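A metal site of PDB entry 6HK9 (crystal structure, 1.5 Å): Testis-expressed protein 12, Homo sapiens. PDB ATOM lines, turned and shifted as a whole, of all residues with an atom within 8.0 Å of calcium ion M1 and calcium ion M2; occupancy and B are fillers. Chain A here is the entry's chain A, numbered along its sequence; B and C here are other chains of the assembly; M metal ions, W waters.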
ATOM      1  N   ASP A   6     -17.622  12.376  31.832  1.00  0.00           N
ATOM      2  CA  ASP A   6     -16.534  12.314  30.869  1.00  0.00           C
ATOM      3  C   ASP A   6     -17.049  11.869  29.513  1.00  0.00           C
ATOM      4  O   ASP A   6     -16.357  11.984  28.508  1.00  0.00           O
ATOM      5  CB  ASP A   6     -15.431  11.376  31.346  1.00  0.00           C
ATOM      6  CG  ASP A   6     -15.810   9.924  31.246  1.00  0.00           C
ATOM      7  OD1 ASP A   6     -16.991   9.605  31.488  1.00  0.00           O
ATOM      8  OD2 ASP A   6     -14.927   9.112  30.910  1.00  0.00           O
ATOM      9  N   GLU A   7     -18.260  11.342  29.483  1.00  0.00           N
ATOM     10  CA  GLU A   7     -18.950  11.044  28.242  1.00  0.00           C
ATOM     11  C   GLU A   7     -19.933  12.164  27.929  1.00  0.00           C
ATOM     12  O   GLU A   7     -20.398  12.889  28.815  1.00  0.00           O
ATOM     13  CB  GLU A   7     -19.663   9.683  28.332  1.00  0.00           C
ATOM     14  CG  GLU A   7     -18.725   8.526  28.667  1.00  0.00           C
ATOM     15  CD  GLU A   7     -19.314   7.155  28.333  1.00  0.00           C
ATOM     16  OE1 GLU A   7     -20.390   6.811  28.865  1.00  0.00           O
ATOM     17  OE2 GLU A   7     -18.683   6.413  27.545  1.00  0.00           O
ATOM     18  N   ALA A   8     -20.242  12.304  26.646  1.00  0.00           N
ATOM     19  CA  ALA A   8     -21.149  13.358  26.211  1.00  0.00           C
ATOM     20  C   ALA A   8     -22.530  13.169  26.847  1.00  0.00           C
ATOM     21  O   ALA A   8     -22.917  12.067  27.201  1.00  0.00           O
ATOM     22  CB  ALA A   8     -21.283  13.338  24.681  1.00  0.00           C
ATOM     23  N   LEU A   9     -23.279  14.274  26.974  1.00  0.00           N
ATOM     24  CA  LEU A   9     -24.626  14.196  27.543  1.00  0.00           C
ATOM     25  C   LEU A   9     -25.497  13.249  26.728  1.00  0.00           C
ATOM     26  O   LEU A   9     -26.350  12.550  27.286  1.00  0.00           O
ATOM     27  CB  LEU A   9     -25.257  15.580  27.598  1.00  0.00           C
ATOM     28  CG  LEU A   9     -24.685  16.535  28.632  1.00  0.00           C
ATOM     29  CD1 LEU A   9     -25.185  17.958  28.421  1.00  0.00           C
ATOM     30  CD2 LEU A   9     -25.029  16.038  30.037  1.00  0.00           C
ATOM     31  N   GLU A  10     -25.298  13.231  25.409  1.00  0.00           N
ATOM     32  CA  GLU A  10     -26.064  12.330  24.535  1.00  0.00           C
ATOM     33  C   GLU A  10     -25.770  10.882  24.869  1.00  0.00           C
ATOM     34  O   GLU A  10     -26.680  10.038  24.811  1.00  0.00           O
ATOM     35  CB  GLU A  10     -25.678  12.602  23.081  1.00  0.00           C
ATOM     36  CG  GLU A  10     -26.072  13.948  22.558  1.00  0.00           C
ATOM     37  CD  GLU A  10     -24.920  14.964  22.580  1.00  0.00           C
ATOM     38  OE1 GLU A  10     -24.045  14.856  23.455  1.00  0.00           O
ATOM     39  OE2 GLU A  10     -24.866  15.877  21.718  1.00  0.00           O
ATOM     40  N   LYS A  11     -24.510  10.568  25.147  1.00  0.00           N
ATOM     41  CA  LYS A  11     -24.132   9.212  25.523  1.00  0.00           C
ATOM     42  C   LYS A  11     -24.703   8.861  26.876  1.00  0.00           C
ATOM     43  O   LYS A  11     -25.228   7.758  27.085  1.00  0.00           O
ATOM     44  CB  LYS A  11     -22.612   9.091  25.551  1.00  0.00           C
ATOM     45  CG  LYS A  11     -22.057   7.788  26.089  1.00  0.00           C
ATOM     46  CD  LYS A  11     -22.557   6.587  25.291  1.00  0.00           C
ATOM     47  CE  LYS A  11     -21.738   5.329  25.577  1.00  0.00           C
ATOM     48  NZ  LYS A  11     -21.614   5.010  27.033  1.00  0.00           N
ATOM     49  N   ASP A  12     -24.629   9.807  27.825  1.00  0.00           N
ATOM     50  CA  ASP A  12     -25.136   9.536  29.156  1.00  0.00           C
ATOM     51  C   ASP A  12     -26.653   9.387  29.141  1.00  0.00           C
ATOM     52  O   ASP A  12     -27.203   8.570  29.877  1.00  0.00           O
ATOM     53  CB  ASP A  12     -24.684  10.625  30.138  1.00  0.00           C
ATOM     54  CG  ASP A  12     -23.245  10.456  30.556  1.00  0.00           C
ATOM     55  OD1 ASP A  12     -22.669   9.374  30.291  1.00  0.00           O
ATOM     56  OD2 ASP A  12     -22.655  11.417  31.129  1.00  0.00           O
ATOM     57  N   LEU A  13     -27.338  10.150  28.306  1.00  0.00           N
ATOM     58  CA  LEU A  13     -28.783   9.981  28.176  1.00  0.00           C
ATOM     59  C   LEU A  13     -29.128   8.588  27.678  1.00  0.00           C
ATOM     60  O   LEU A  13     -30.124   7.987  28.100  1.00  0.00           O
ATOM     61  CB  LEU A  13     -29.357  11.035  27.239  1.00  0.00           C
ATOM     62  CG  LEU A  13     -30.877  10.967  27.091  1.00  0.00           C
ATOM     63  CD1 LEU A  13     -31.574  11.014  28.454  1.00  0.00           C
ATOM     64  CD2 LEU A  13     -31.324  12.113  26.196  1.00  0.00           C
ATOM     65  N   ASN A  14     -28.331   8.059  26.755  1.00  0.00           N
ATOM     66  CA  ASN A  14     -28.590   6.735  26.218  1.00  0.00           C
ATOM     67  C   ASN A  14     -28.266   5.670  27.258  1.00  0.00           C
ATOM     68  O   ASN A  14     -28.979   4.651  27.349  1.00  0.00           O
ATOM     69  CB  ASN A  14     -27.767   6.528  24.957  1.00  0.00           C
ATOM     70  CG  ASN A  14     -28.262   5.354  24.143  1.00  0.00           C
ATOM     71  OD1 ASN A  14     -27.656   4.276  24.158  1.00  0.00           O
ATOM     72  ND2 ASN A  14     -29.381   5.544  23.443  1.00  0.00           N
ATOM     73  N   ASP A  15     -27.232   5.887  28.069  1.00  0.00           N
ATOM     74  CA  ASP A  15     -26.940   4.920  29.130  1.00  0.00           C
ATOM     75  C   ASP A  15     -28.071   4.840  30.143  1.00  0.00           C
ATOM     76  O   ASP A  15     -28.474   3.747  30.562  1.00  0.00           O
ATOM     77  CB  ASP A  15     -25.662   5.306  29.859  1.00  0.00           C
ATOM     78  CG  ASP A  15     -24.429   5.222  28.986  1.00  0.00           C
ATOM     79  OD1 ASP A  15     -24.418   4.382  28.057  1.00  0.00           O
ATOM     80  OD2 ASP A  15     -23.478   5.990  29.246  1.00  0.00           O
ATOM     81  N   VAL A  16     -28.570   5.981  30.610  1.00  0.00           N
ATOM     82  CA  VAL A  16     -29.598   5.940  31.639  1.00  0.00           C
ATOM     83  C   VAL A  16     -30.895   5.380  31.062  1.00  0.00           C
ATOM     84  O   VAL A  16     -31.655   4.683  31.764  1.00  0.00           O
ATOM     85  CB  VAL A  16     -29.805   7.319  32.300  1.00  0.00           C
ATOM     86  CG1 VAL A  16     -30.354   8.301  31.290  1.00  0.00           C
ATOM     87  CG2 VAL A  16     -30.750   7.167  33.493  1.00  0.00           C
ATOM     88  N   GLU A  19     -30.716   1.748  31.439  1.00  0.00           N
ATOM     89  CA  GLU A  19     -30.960   1.359  32.818  1.00  0.00           C
ATOM     90  C   GLU A  19     -32.445   1.359  33.134  1.00  0.00           C
ATOM     91  O   GLU A  19     -32.943   0.454  33.797  1.00  0.00           O
ATOM     92  CB  GLU A  19     -30.256   2.308  33.778  1.00  0.00           C
ATOM     93  CG  GLU A  19     -28.741   2.200  33.845  1.00  0.00           C
ATOM     94  CD  GLU A  19     -28.182   2.907  35.089  1.00  0.00           C
ATOM     95  OE1 GLU A  19     -28.209   2.275  36.190  1.00  0.00           O
ATOM     96  OE2 GLU A  19     -27.762   4.082  34.960  1.00  0.00           O
ATOM     97  N   ASP B   6     -19.111  14.760  34.349  1.00  0.00           N
ATOM     98  CA  ASP B   6     -19.374  16.182  34.513  1.00  0.00           C
ATOM     99  C   ASP B   6     -18.831  16.673  35.841  1.00  0.00           C
ATOM    100  O   ASP B   6     -18.726  17.872  36.073  1.00  0.00           O
ATOM    101  CB  ASP B   6     -20.866  16.479  34.413  1.00  0.00           C
ATOM    102  CG  ASP B   6     -21.637  16.037  35.627  1.00  0.00           C
ATOM    103  OD1 ASP B   6     -21.290  14.981  36.193  1.00  0.00           O
ATOM    104  OD2 ASP B   6     -22.575  16.757  36.017  1.00  0.00           O
ATOM    105  N   GLU B   7     -18.492  15.745  36.727  1.00  0.00           N
ATOM    106  CA  GLU B   7     -17.802  16.062  37.957  1.00  0.00           C
ATOM    107  C   GLU B   7     -16.318  15.767  37.785  1.00  0.00           C
ATOM    108  O   GLU B   7     -15.908  14.950  36.952  1.00  0.00           O
ATOM    109  CB  GLU B   7     -18.396  15.269  39.134  1.00  0.00           C
ATOM    110  CG  GLU B   7     -19.890  15.510  39.338  1.00  0.00           C
ATOM    111  CD  GLU B   7     -20.386  15.094  40.723  1.00  0.00           C
ATOM    112  OE1 GLU B   7     -20.237  13.910  41.090  1.00  0.00           O
ATOM    113  OE2 GLU B   7     -20.934  15.954  41.442  1.00  0.00           O
ATOM    114  N   GLU C  51     -32.640  11.431  36.944  1.00  0.00           N
ATOM    115  CA  GLU C  51     -31.332  11.539  36.320  1.00  0.00           C
ATOM    116  C   GLU C  51     -31.470  11.673  34.801  1.00  0.00           C
ATOM    117  O   GLU C  51     -30.790  12.504  34.178  1.00  0.00           O
ATOM    118  CB  GLU C  51     -30.484  10.314  36.669  1.00  0.00           C
ATOM    119  CG  GLU C  51     -29.320  10.132  35.735  1.00  0.00           C
ATOM    120  CD  GLU C  51     -28.242   9.201  36.266  1.00  0.00           C
ATOM    121  OE1 GLU C  51     -28.578   8.261  37.016  1.00  0.00           O
ATOM    122  OE2 GLU C  51     -27.065   9.421  35.896  1.00  0.00           O
ATOM    123  N   ILE C  55     -30.237  14.894  32.490  1.00  0.00           N
ATOM    124  CA  ILE C  55     -29.355  14.767  31.336  1.00  0.00           C
ATOM    125  C   ILE C  55     -30.038  15.295  30.083  1.00  0.00           C
ATOM    126  O   ILE C  55     -29.430  16.007  29.272  1.00  0.00           O
ATOM    127  CB  ILE C  55     -28.907  13.308  31.144  1.00  0.00           C
ATOM    128  CG1 ILE C  55     -28.107  12.816  32.357  1.00  0.00           C
ATOM    129  CG2 ILE C  55     -28.093  13.178  29.871  1.00  0.00           C
ATOM    130  CD1 ILE C  55     -27.926  11.322  32.364  1.00  0.00           C
ATOM    131  N   LYS C  62     -27.244  22.183  25.800  1.00  0.00           N
ATOM    132  CA  LYS C  62     -25.985  22.071  25.062  1.00  0.00           C
ATOM    133  C   LYS C  62     -26.189  22.405  23.594  1.00  0.00           C
ATOM    134  O   LYS C  62     -25.370  23.118  22.979  1.00  0.00           O
ATOM    135  CB  LYS C  62     -25.473  20.646  25.192  1.00  0.00           C
ATOM    136  CG  LYS C  62     -24.356  20.312  24.197  1.00  0.00           C
ATOM    137  CD  LYS C  62     -23.894  18.880  24.376  1.00  0.00           C
ATOM    138  CE  LYS C  62     -22.887  18.486  23.320  1.00  0.00           C
ATOM    139  NZ  LYS C  62     -22.401  17.103  23.563  1.00  0.00           N
HETATM  140 CA    CA M   1     -21.923   7.140  30.668  1.00  0.00          CA
HETATM  141 CA    CA M   2     -20.379  15.039  30.198  1.00  0.00          CA
HETATM  142 CA    CA M   3     -14.973  14.373  34.644  1.00  0.00          CA
HETATM  143  O   HOH W   1     -19.214  14.007  31.826  1.00  0.00           O
HETATM  144  O   HOH W   2     -21.510   5.267  31.760  1.00  0.00           O
HETATM  145  O   HOH W   3     -22.266  13.904  31.018  1.00  0.00           O
HETATM  146  O   HOH W   4     -20.245   7.951  32.020  1.00  0.00           O
HETATM  147  O   HOH W   5     -23.553   7.133  32.203  1.00  0.00           O
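NZ of Lys 11 is in salt-bridge range of OD1 of Asp 15 (3.1 Å).
The side-chain amino group of Lys 11 is in salt-bridge range of the side-chain carboxylate of Glu 7 of chain A (3.3 Å).
Of the 17 residues printed, 1 comes within 4 Å of calcium ion M2.
Of the 17 residues printed, 3 come within 4 Å of calcium ion M1.
The nearest printed residue that does not touch calcium ion M1 is Lys 11 (4.2 Å).
Water W1 is bound to calcium ion M2, at 2.3 Å.
Calcium ion M2 is bound by water W3 (2.3 Å).
Calcium ion M2 is bound by the backbone carbonyl oxygen (O) of Glu 7 of chain A, 2.6 Å away.
Calcium ion M2 has three donor atoms within binding distance.
Calcium ion M1 is bound by water W2 (2.2 Å), water W5 (2.2 Å), water W4 (2.3 Å), the side-chain carboxylate of Asp 12 (2.4 Å), the side-chain carboxylate of Glu 7 of chain A (2.4 Å) and the side-chain carboxylate of Asp 15 (2.4 Å).
Calcium ion M1 has six donor atoms within binding distance.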
